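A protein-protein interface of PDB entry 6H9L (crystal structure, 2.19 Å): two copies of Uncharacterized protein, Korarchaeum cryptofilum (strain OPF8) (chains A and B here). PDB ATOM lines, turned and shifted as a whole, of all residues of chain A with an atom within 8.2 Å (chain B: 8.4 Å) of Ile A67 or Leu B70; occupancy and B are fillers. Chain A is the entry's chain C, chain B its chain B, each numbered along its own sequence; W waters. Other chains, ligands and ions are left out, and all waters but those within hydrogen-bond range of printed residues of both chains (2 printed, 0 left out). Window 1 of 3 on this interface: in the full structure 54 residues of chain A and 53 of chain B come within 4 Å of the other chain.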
ATOM      1  N   ARG A  60     -29.546 -17.064  21.413  1.00  0.00           N
ATOM      2  CA  ARG A  60     -28.658 -15.918  21.268  1.00  0.00           C
ATOM      3  C   ARG A  60     -27.928 -15.625  22.579  1.00  0.00           C
ATOM      4  O   ARG A  60     -26.706 -15.453  22.604  1.00  0.00           O
ATOM      5  CB  ARG A  60     -29.451 -14.684  20.837  1.00  0.00           C
ATOM      6  CG  ARG A  60     -28.561 -13.511  20.441  1.00  0.00           C
ATOM      7  CD  ARG A  60     -29.349 -12.241  20.224  1.00  0.00           C
ATOM      8  NE  ARG A  60     -29.772 -12.151  18.826  1.00  0.00           N
ATOM      9  CZ  ARG A  60     -30.942 -12.552  18.310  1.00  0.00           C
ATOM     10  NH1 ARG A  60     -31.910 -13.087  19.058  1.00  0.00           N
ATOM     11  NH2 ARG A  60     -31.150 -12.402  17.007  1.00  0.00           N
ATOM     12  N   LYS A  61     -28.692 -15.577  23.663  1.00  0.00           N
ATOM     13  CA  LYS A  61     -28.147 -15.313  24.990  1.00  0.00           C
ATOM     14  C   LYS A  61     -27.131 -16.389  25.409  1.00  0.00           C
ATOM     15  O   LYS A  61     -26.048 -16.073  25.897  1.00  0.00           O
ATOM     16  CB  LYS A  61     -29.296 -15.222  25.994  1.00  0.00           C
ATOM     17  CG  LYS A  61     -28.920 -14.743  27.386  1.00  0.00           C
ATOM     18  CD  LYS A  61     -30.173 -14.665  28.258  1.00  0.00           C
ATOM     19  CE  LYS A  61     -29.900 -14.072  29.636  1.00  0.00           C
ATOM     20  NZ  LYS A  61     -29.000 -14.923  30.465  1.00  0.00           N
ATOM     21  N   ALA A  62     -27.475 -17.655  25.194  1.00  0.00           N
ATOM     22  CA  ALA A  62     -26.576 -18.770  25.525  1.00  0.00           C
ATOM     23  C   ALA A  62     -25.291 -18.768  24.683  1.00  0.00           C
ATOM     24  O   ALA A  62     -24.194 -19.043  25.190  1.00  0.00           O
ATOM     25  CB  ALA A  62     -27.304 -20.094  25.362  1.00  0.00           C
ATOM     26  N   THR A  63     -25.432 -18.453  23.402  1.00  0.00           N
ATOM     27  CA  THR A  63     -24.283 -18.377  22.495  1.00  0.00           C
ATOM     28  C   THR A  63     -23.315 -17.276  22.921  1.00  0.00           C
ATOM     29  O   THR A  63     -22.097 -17.480  22.989  1.00  0.00           O
ATOM     30  CB  THR A  63     -24.754 -18.142  21.057  1.00  0.00           C
ATOM     31  OG1 THR A  63     -25.494 -19.283  20.617  1.00  0.00           O
ATOM     32  CG2 THR A  63     -23.579 -17.907  20.112  1.00  0.00           C
ATOM     33  N   LYS A  64     -23.867 -16.103  23.199  1.00  0.00           N
ATOM     34  CA  LYS A  64     -23.068 -14.978  23.661  1.00  0.00           C
ATOM     35  C   LYS A  64     -22.250 -15.339  24.906  1.00  0.00           C
ATOM     36  O   LYS A  64     -21.062 -15.021  25.004  1.00  0.00           O
ATOM     37  CB  LYS A  64     -23.970 -13.775  23.935  1.00  0.00           C
ATOM     38  CG  LYS A  64     -23.205 -12.523  24.317  1.00  0.00           C
ATOM     39  CD  LYS A  64     -24.106 -11.305  24.323  1.00  0.00           C
ATOM     40  CE  LYS A  64     -23.366 -10.093  24.832  1.00  0.00           C
ATOM     41  NZ  LYS A  64     -24.250  -8.897  24.854  1.00  0.00           N
ATOM     42  N   GLU A  65     -22.884 -16.015  25.848  1.00  0.00           N
ATOM     43  CA  GLU A  65     -22.178 -16.472  27.035  1.00  0.00           C
ATOM     44  C   GLU A  65     -21.097 -17.515  26.753  1.00  0.00           C
ATOM     45  O   GLU A  65     -20.029 -17.500  27.375  1.00  0.00           O
ATOM     46  CB  GLU A  65     -23.162 -17.080  28.029  1.00  0.00           C
ATOM     47  CG  GLU A  65     -22.494 -17.513  29.325  1.00  0.00           C
ATOM     48  CD  GLU A  65     -23.469 -17.689  30.471  1.00  0.00           C
ATOM     49  OE1 GLU A  65     -24.684 -17.580  30.219  1.00  0.00           O
ATOM     50  OE2 GLU A  65     -23.024 -17.950  31.615  1.00  0.00           O
ATOM     51  N   ASP A  66     -21.406 -18.450  25.863  1.00  0.00           N
ATOM     52  CA  ASP A  66     -20.459 -19.514  25.508  1.00  0.00           C
ATOM     53  C   ASP A  66     -19.214 -18.946  24.832  1.00  0.00           C
ATOM     54  O   ASP A  66     -18.089 -19.387  25.102  1.00  0.00           O
ATOM     55  CB  ASP A  66     -21.117 -20.542  24.580  1.00  0.00           C
ATOM     56  CG  ASP A  66     -22.134 -21.416  25.291  1.00  0.00           C
ATOM     57  OD1 ASP A  66     -22.109 -21.484  26.534  1.00  0.00           O
ATOM     58  OD2 ASP A  66     -22.965 -22.046  24.601  1.00  0.00           O
ATOM     59  N   ILE A  67     -19.418 -17.951  23.977  1.00  0.00           N
ATOM     60  CA  ILE A  67     -18.303 -17.260  23.336  1.00  0.00           C
ATOM     61  C   ILE A  67     -17.482 -16.465  24.361  1.00  0.00           C
ATOM     62  O   ILE A  67     -16.258 -16.476  24.308  1.00  0.00           O
ATOM     63  CB  ILE A  67     -18.791 -16.340  22.198  1.00  0.00           C
ATOM     64  CG1 ILE A  67     -19.347 -17.194  21.058  1.00  0.00           C
ATOM     65  CG2 ILE A  67     -17.659 -15.467  21.683  1.00  0.00           C
ATOM     66  CD1 ILE A  67     -20.024 -16.405  19.953  1.00  0.00           C
ATOM     67  N   GLU A  68     -18.155 -15.763  25.270  1.00  0.00           N
ATOM     68  CA  GLU A  68     -17.461 -14.998  26.303  1.00  0.00           C
ATOM     69  C   GLU A  68     -16.621 -15.894  27.228  1.00  0.00           C
ATOM     70  O   GLU A  68     -15.508 -15.523  27.594  1.00  0.00           O
ATOM     71  CB  GLU A  68     -18.455 -14.147  27.103  1.00  0.00           C
ATOM     72  CG  GLU A  68     -17.836 -13.326  28.227  1.00  0.00           C
ATOM     73  CD  GLU A  68     -16.933 -12.186  27.740  1.00  0.00           C
ATOM     74  OE1 GLU A  68     -16.344 -11.464  28.586  1.00  0.00           O
ATOM     75  OE2 GLU A  68     -16.795 -12.002  26.514  1.00  0.00           O
ATOM     76  N   ASP A  69     -17.170 -17.052  27.601  1.00  0.00           N
ATOM     77  CA  ASP A  69     -16.431 -18.054  28.376  1.00  0.00           C
ATOM     78  C   ASP A  69     -15.125 -18.462  27.678  1.00  0.00           C
ATOM     79  O   ASP A  69     -14.054 -18.498  28.306  1.00  0.00           O
ATOM     80  CB  ASP A  69     -17.308 -19.303  28.655  1.00  0.00           C
ATOM     81  CG  ASP A  69     -18.286 -19.117  29.810  1.00  0.00           C
ATOM     82  OD1 ASP A  69     -18.212 -18.161  30.612  1.00  0.00           O
ATOM     83  OD2 ASP A  69     -19.164 -19.979  29.923  1.00  0.00           O
ATOM     84  N   LEU A  70     -15.200 -18.710  26.377  1.00  0.00           N
ATOM     85  CA  LEU A  70     -14.011 -19.091  25.617  1.00  0.00           C
ATOM     86  C   LEU A  70     -13.016 -17.933  25.490  1.00  0.00           C
ATOM     87  O   LEU A  70     -11.802 -18.141  25.616  1.00  0.00           O
ATOM     88  CB  LEU A  70     -14.389 -19.614  24.234  1.00  0.00           C
ATOM     89  CG  LEU A  70     -13.212 -20.036  23.338  1.00  0.00           C
ATOM     90  CD1 LEU A  70     -12.292 -21.044  24.031  1.00  0.00           C
ATOM     91  CD2 LEU A  70     -13.710 -20.600  22.022  1.00  0.00           C
ATOM     92  N   ARG A  71     -13.514 -16.723  25.234  1.00  0.00           N
ATOM     93  CA  ARG A  71     -12.644 -15.547  25.155  1.00  0.00           C
ATOM     94  C   ARG A  71     -11.845 -15.409  26.449  1.00  0.00           C
ATOM     95  O   ARG A  71     -10.647 -15.155  26.424  1.00  0.00           O
ATOM     96  CB  ARG A  71     -13.441 -14.252  24.928  1.00  0.00           C
ATOM     97  CG  ARG A  71     -12.548 -13.015  24.769  1.00  0.00           C
ATOM     98  CD  ARG A  71     -13.298 -11.681  24.797  1.00  0.00           C
ATOM     99  NE  ARG A  71     -13.812 -11.303  26.115  1.00  0.00           N
ATOM    100  CZ  ARG A  71     -13.077 -10.850  27.136  1.00  0.00           C
ATOM    101  NH1 ARG A  71     -11.758 -10.730  27.043  1.00  0.00           N
ATOM    102  NH2 ARG A  71     -13.671 -10.532  28.281  1.00  0.00           N
ATOM    103  N   GLU A  72     -12.538 -15.577  27.573  1.00  0.00           N
ATOM    104  CA  GLU A  72     -11.939 -15.359  28.884  1.00  0.00           C
ATOM    105  C   GLU A  72     -10.917 -16.463  29.219  1.00  0.00           C
ATOM    106  O   GLU A  72      -9.799 -16.180  29.662  1.00  0.00           O
ATOM    107  CB  GLU A  72     -13.046 -15.156  29.944  1.00  0.00           C
ATOM    108  CG  GLU A  72     -13.411 -13.689  30.130  1.00  0.00           C
ATOM    109  CD  GLU A  72     -14.217 -13.422  31.388  1.00  0.00           C
ATOM    110  OE1 GLU A  72     -15.414 -13.770  31.443  1.00  0.00           O
ATOM    111  OE2 GLU A  72     -13.634 -12.841  32.314  1.00  0.00           O
ATOM    112  N   ALA A  73     -11.268 -17.708  28.932  1.00  0.00           N
ATOM    113  CA  ALA A  73     -10.328 -18.826  29.086  1.00  0.00           C
ATOM    114  C   ALA A  73      -9.087 -18.655  28.197  1.00  0.00           C
ATOM    115  O   ALA A  73      -7.949 -18.863  28.641  1.00  0.00           O
ATOM    116  CB  ALA A  73     -11.033 -20.129  28.745  1.00  0.00           C
ATOM    117  N   THR A  74      -9.313 -18.294  26.935  1.00  0.00           N
ATOM    118  CA  THR A  74      -8.222 -18.070  25.976  1.00  0.00           C
ATOM    119  C   THR A  74      -7.259 -16.989  26.460  1.00  0.00           C
ATOM    120  O   THR A  74      -6.042 -17.135  26.350  1.00  0.00           O
ATOM    121  CB  THR A  74      -8.777 -17.664  24.611  1.00  0.00           C
ATOM    122  OG1 THR A  74      -9.508 -18.762  24.061  1.00  0.00           O
ATOM    123  CG2 THR A  74      -7.666 -17.272  23.626  1.00  0.00           C
ATOM    124  N   LYS A  75      -7.811 -15.894  26.972  1.00  0.00           N
ATOM    125  CA  LYS A  75      -7.001 -14.814  27.507  1.00  0.00           C
ATOM    126  C   LYS A  75      -6.121 -15.316  28.665  1.00  0.00           C
ATOM    127  O   LYS A  75      -4.957 -14.938  28.779  1.00  0.00           O
ATOM    128  CB  LYS A  75      -7.893 -13.656  27.958  1.00  0.00           C
ATOM    129  CG  LYS A  75      -7.148 -12.515  28.623  1.00  0.00           C
ATOM    130  CD  LYS A  75      -8.092 -11.402  29.027  1.00  0.00           C
ATOM    131  CE  LYS A  75      -7.404 -10.429  29.956  1.00  0.00           C
ATOM    132  NZ  LYS A  75      -8.222  -9.214  30.191  1.00  0.00           N
ATOM    133  N   ALA B  62     -25.096 -13.476  12.820  1.00  0.00           N
ATOM    134  CA  ALA B  62     -24.470 -12.837  13.981  1.00  0.00           C
ATOM    135  C   ALA B  62     -23.519 -13.775  14.718  1.00  0.00           C
ATOM    136  O   ALA B  62     -22.436 -13.359  15.152  1.00  0.00           O
ATOM    137  CB  ALA B  62     -25.539 -12.314  14.941  1.00  0.00           C
ATOM    138  N   THR B  63     -23.930 -15.030  14.875  1.00  0.00           N
ATOM    139  CA  THR B  63     -23.115 -16.023  15.561  1.00  0.00           C
ATOM    140  C   THR B  63     -21.819 -16.283  14.803  1.00  0.00           C
ATOM    141  O   THR B  63     -20.727 -16.294  15.394  1.00  0.00           O
ATOM    142  CB  THR B  63     -23.880 -17.340  15.715  1.00  0.00           C
ATOM    143  OG1 THR B  63     -24.992 -17.123  16.581  1.00  0.00           O
ATOM    144  CG2 THR B  63     -23.008 -18.432  16.314  1.00  0.00           C
ATOM    145  N   LYS B  64     -21.948 -16.495  13.497  1.00  0.00           N
ATOM    146  CA  LYS B  64     -20.799 -16.710  12.639  1.00  0.00           C
ATOM    147  C   LYS B  64     -19.806 -15.556  12.766  1.00  0.00           C
ATOM    148  O   LYS B  64     -18.606 -15.781  12.889  1.00  0.00           O
ATOM    149  CB  LYS B  64     -21.237 -16.866  11.181  1.00  0.00           C
ATOM    150  CG  LYS B  64     -20.094 -17.204  10.248  1.00  0.00           C
ATOM    151  CD  LYS B  64     -20.596 -17.611   8.879  1.00  0.00           C
ATOM    152  CE  LYS B  64     -19.450 -17.808   7.918  1.00  0.00           C
ATOM    153  NZ  LYS B  64     -19.938 -18.199   6.571  1.00  0.00           N
ATOM    154  N   GLU B  65     -20.311 -14.328  12.742  1.00  0.00           N
ATOM    155  CA  GLU B  65     -19.461 -13.145  12.908  1.00  0.00           C
ATOM    156  C   GLU B  65     -18.798 -13.060  14.289  1.00  0.00           C
ATOM    157  O   GLU B  65     -17.635 -12.692  14.396  1.00  0.00           O
ATOM    158  CB  GLU B  65     -20.251 -11.862  12.627  1.00  0.00           C
ATOM    159  CG  GLU B  65     -20.517 -11.656  11.144  1.00  0.00           C
ATOM    160  CD  GLU B  65     -21.664 -10.696  10.887  1.00  0.00           C
ATOM    161  OE1 GLU B  65     -22.208 -10.160  11.872  1.00  0.00           O
ATOM    162  OE2 GLU B  65     -22.038 -10.470   9.712  1.00  0.00           O
ATOM    163  N   ASP B  66     -19.548 -13.396  15.338  1.00  0.00           N
ATOM    164  CA  ASP B  66     -19.030 -13.347  16.702  1.00  0.00           C
ATOM    165  C   ASP B  66     -17.914 -14.365  16.908  1.00  0.00           C
ATOM    166  O   ASP B  66     -16.908 -14.082  17.576  1.00  0.00           O
ATOM    167  CB  ASP B  66     -20.151 -13.608  17.716  1.00  0.00           C
ATOM    168  CG  ASP B  66     -21.126 -12.449  17.832  1.00  0.00           C
ATOM    169  OD1 ASP B  66     -20.792 -11.327  17.415  1.00  0.00           O
ATOM    170  OD2 ASP B  66     -22.236 -12.669  18.368  1.00  0.00           O
ATOM    171  N   ILE B  67     -18.098 -15.557  16.342  1.00  0.00           N
ATOM    172  CA  ILE B  67     -17.065 -16.596  16.392  1.00  0.00           C
ATOM    173  C   ILE B  67     -15.840 -16.185  15.578  1.00  0.00           C
ATOM    174  O   ILE B  67     -14.705 -16.390  16.016  1.00  0.00           O
ATOM    175  CB  ILE B  67     -17.600 -17.960  15.901  1.00  0.00           C
ATOM    176  CG1 ILE B  67     -18.647 -18.490  16.882  1.00  0.00           C
ATOM    177  CG2 ILE B  67     -16.460 -18.969  15.757  1.00  0.00           C
ATOM    178  CD1 ILE B  67     -19.374 -19.733  16.409  1.00  0.00           C
ATOM    179  N   GLU B  68     -16.059 -15.617  14.395  1.00  0.00           N
ATOM    180  CA  GLU B  68     -14.959 -15.161  13.551  1.00  0.00           C
ATOM    181  C   GLU B  68     -14.155 -14.064  14.228  1.00  0.00           C
ATOM    182  O   GLU B  68     -12.939 -14.050  14.139  1.00  0.00           O
ATOM    183  CB  GLU B  68     -15.464 -14.704  12.184  1.00  0.00           C
ATOM    184  CG  GLU B  68     -14.385 -14.144  11.257  1.00  0.00           C
ATOM    185  CD  GLU B  68     -13.261 -15.108  10.927  1.00  0.00           C
ATOM    186  OE1 GLU B  68     -13.351 -16.302  11.273  1.00  0.00           O
ATOM    187  OE2 GLU B  68     -12.256 -14.651  10.327  1.00  0.00           O
ATOM    188  N   ASP B  69     -14.840 -13.133  14.880  1.00  0.00           N
ATOM    189  CA  ASP B  69     -14.166 -12.112  15.660  1.00  0.00           C
ATOM    190  C   ASP B  69     -13.243 -12.711  16.708  1.00  0.00           C
ATOM    191  O   ASP B  69     -12.133 -12.243  16.867  1.00  0.00           O
ATOM    192  CB  ASP B  69     -15.174 -11.235  16.356  1.00  0.00           C
ATOM    193  CG  ASP B  69     -14.509 -10.189  17.245  1.00  0.00           C
ATOM    194  OD1 ASP B  69     -13.648  -9.482  16.693  1.00  0.00           O
ATOM    195  OD2 ASP B  69     -14.799 -10.093  18.471  1.00  0.00           O
ATOM    196  N   LEU B  70     -13.715 -13.726  17.425  1.00  0.00           N
ATOM    197  CA  LEU B  70     -12.894 -14.361  18.455  1.00  0.00           C
ATOM    198  C   LEU B  70     -11.714 -15.119  17.854  1.00  0.00           C
ATOM    199  O   LEU B  70     -10.599 -15.057  18.383  1.00  0.00           O
ATOM    200  CB  LEU B  70     -13.727 -15.289  19.347  1.00  0.00           C
ATOM    201  CG  LEU B  70     -12.946 -16.018  20.451  1.00  0.00           C
ATOM    202  CD1 LEU B  70     -12.156 -15.059  21.336  1.00  0.00           C
ATOM    203  CD2 LEU B  70     -13.883 -16.850  21.307  1.00  0.00           C
ATOM    204  N   ARG B  71     -11.955 -15.830  16.760  1.00  0.00           N
ATOM    205  CA  ARG B  71     -10.874 -16.515  16.061  1.00  0.00           C
ATOM    206  C   ARG B  71      -9.786 -15.521  15.681  1.00  0.00           C
ATOM    207  O   ARG B  71      -8.606 -15.790  15.865  1.00  0.00           O
ATOM    208  CB  ARG B  71     -11.367 -17.211  14.789  1.00  0.00           C
ATOM    209  CG  ARG B  71     -10.265 -18.007  14.082  1.00  0.00           C
ATOM    210  CD  ARG B  71     -10.651 -18.461  12.684  1.00  0.00           C
ATOM    211  NE  ARG B  71     -10.713 -17.298  11.793  1.00  0.00           N
ATOM    212  CZ  ARG B  71      -9.660 -16.674  11.252  1.00  0.00           C
ATOM    213  NH1 ARG B  71      -8.422 -17.095  11.480  1.00  0.00           N
ATOM    214  NH2 ARG B  71      -9.844 -15.619  10.464  1.00  0.00           N
ATOM    215  N   GLU B  72     -10.209 -14.377  15.151  1.00  0.00           N
ATOM    216  CA  GLU B  72      -9.290 -13.363  14.661  1.00  0.00           C
ATOM    217  C   GLU B  72      -8.517 -12.720  15.809  1.00  0.00           C
ATOM    218  O   GLU B  72      -7.309 -12.545  15.717  1.00  0.00           O
ATOM    219  CB  GLU B  72     -10.037 -12.270  13.893  1.00  0.00           C
ATOM    220  CG  GLU B  72      -9.546 -12.090  12.467  1.00  0.00           C
ATOM    221  CD  GLU B  72      -9.940 -10.754  11.878  1.00  0.00           C
ATOM    222  OE1 GLU B  72     -11.132 -10.543  11.569  1.00  0.00           O
ATOM    223  OE2 GLU B  72      -9.043  -9.916  11.705  1.00  0.00           O
ATOM    224  N   ALA B  73      -9.224 -12.367  16.876  1.00  0.00           N
ATOM    225  CA  ALA B  73      -8.599 -11.796  18.061  1.00  0.00           C
ATOM    226  C   ALA B  73      -7.577 -12.767  18.658  1.00  0.00           C
ATOM    227  O   ALA B  73      -6.460 -12.373  18.988  1.00  0.00           O
ATOM    228  CB  ALA B  73      -9.656 -11.453  19.095  1.00  0.00           C
ATOM    229  N   THR B  74      -7.974 -14.033  18.778  1.00  0.00           N
ATOM    230  CA  THR B  74      -7.107 -15.073  19.312  1.00  0.00           C
ATOM    231  C   THR B  74      -5.827 -15.220  18.482  1.00  0.00           C
ATOM    232  O   THR B  74      -4.727 -15.325  19.036  1.00  0.00           O
ATOM    233  CB  THR B  74      -7.835 -16.430  19.353  1.00  0.00           C
ATOM    234  OG1 THR B  74      -8.934 -16.358  20.272  1.00  0.00           O
ATOM    235  CG2 THR B  74      -6.887 -17.544  19.779  1.00  0.00           C
ATOM    236  N   LYS B  75      -5.982 -15.232  17.163  1.00  0.00           N
ATOM    237  CA  LYS B  75      -4.840 -15.308  16.259  1.00  0.00           C
ATOM    238  C   LYS B  75      -3.898 -14.118  16.471  1.00  0.00           C
ATOM    239  O   LYS B  75      -2.684 -14.282  16.469  1.00  0.00           O
ATOM    240  CB  LYS B  75      -5.313 -15.364  14.801  1.00  0.00           C
ATOM    241  CG  LYS B  75      -4.189 -15.339  13.775  1.00  0.00           C
ATOM    242  CD  LYS B  75      -4.705 -15.383  12.345  1.00  0.00           C
ATOM    243  CE  LYS B  75      -3.592 -14.967  11.361  1.00  0.00           C
ATOM    244  NZ  LYS B  75      -3.510 -13.478  11.213  1.00  0.00           N
ATOM    245  N   GLU B  76      -4.461 -12.928  16.665  1.00  0.00           N
ATOM    246  CA  GLU B  76      -3.662 -11.719  16.889  1.00  0.00           C
ATOM    247  C   GLU B  76      -2.950 -11.748  18.238  1.00  0.00           C
ATOM    248  O   GLU B  76      -1.812 -11.316  18.339  1.00  0.00           O
ATOM    249  CB  GLU B  76      -4.525 -10.462  16.806  1.00  0.00           C
ATOM    250  CG  GLU B  76      -5.069 -10.167  15.419  1.00  0.00           C
ATOM    251  CD  GLU B  76      -6.120  -9.065  15.419  1.00  0.00           C
ATOM    252  OE1 GLU B  76      -6.248  -8.369  16.445  1.00  0.00           O
ATOM    253  OE2 GLU B  76      -6.821  -8.880  14.403  1.00  0.00           O
ATOM    254  N   ASP B  77      -3.633 -12.235  19.270  1.00  0.00           N
ATOM    255  CA  ASP B  77      -3.064 -12.302  20.614  1.00  0.00           C
ATOM    256  C   ASP B  77      -1.897 -13.289  20.666  1.00  0.00           C
ATOM    257  O   ASP B  77      -0.864 -13.019  21.286  1.00  0.00           O
ATOM    258  CB  ASP B  77      -4.130 -12.703  21.644  1.00  0.00           C
ATOM    259  CG  ASP B  77      -5.202 -11.647  21.823  1.00  0.00           C
ATOM    260  OD1 ASP B  77      -4.974 -10.479  21.451  1.00  0.00           O
ATOM    261  OD2 ASP B  77      -6.286 -11.986  22.343  1.00  0.00           O
HETATM  262  O   HOH W   1     -25.971 -19.391  17.783  1.00  0.00           O
HETATM  263  O   HOH W   2      -9.970 -18.838  21.379  1.00  0.00           O
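The backbone carbonyl oxygen of Leu B70 sits at hydrogen-bond distance from the side-chain hydroxyl of Thr B74, at 2.8 Å.
The guanidinium group (NH2) of Arg A71 lies within salt-bridge range of the side-chain carboxylate (OE1) of Glu A68.
The side-chain hydroxyl of Thr A74 lies within hydrogen-bond range of the backbone carbonyl oxygen of Leu A70, at 2.8 Å.
Among the printed residues, pairs that only touch across the chains: Ile A67 with Asp B66 (3.6 Å), Thr A74 with Thr B74 (3.7 Å), Leu A70 with Leu B70 (3.8 Å), Ile A67 with Leu B70 (3.8 Å), Thr A63 with Thr B63 (3.9 Å), Arg A71 with Leu B70 (3.9 Å) and Ile A67 with Ile B67 (3.96 Å).
Ile A67 touches just these residues of chain B: Asp B66, Ile B67 and Leu B70.
Of the printed residues of chain A, Thr B63 touches Thr A63 (3.9 Å).
Printed residues of chain A within 4 Å of Ile B67: Ile A67 (3.96 Å).
Leu B70 touches just these residues of chain A: Ile A67 (3.8 Å), Leu A70 (3.8 Å) and Arg A71 (3.9 Å).
Lys B75 touches none of the printed residues of chain A.
The nearest printed residue of chain A that does not touch Thr B63 is Ile A67 (4.6 Å).
Hydrophobic or aromatic side chains of chain B that line the printed part of chain A: Ile B67 and Leu B70.
Thr A63 touches its own counterpart, Thr B63.
Ile A67 touches Asp B66, but with the chains exchanged Asp A66 does not touch Ile B67 (8.0 Å).
Ile A67 touches its own counterpart, Ile B67.
Thr A74 touches its own counterpart, Thr B74.
Positions printed for both chains: 62, 63, 64, 65, 66, 67, 68, 69, 70, 71, 72, 73, 74 and 75.
Water W2 bridges the side-chain hydroxyl of Thr A74 (2.7 Å) and the side-chain hydroxyl of Thr B74 (2.9 Å).
Water W1 bridges the side-chain hydroxyl of Thr B63 (2.7 Å) and the side-chain hydroxyl of Thr A63 (2.9 Å).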
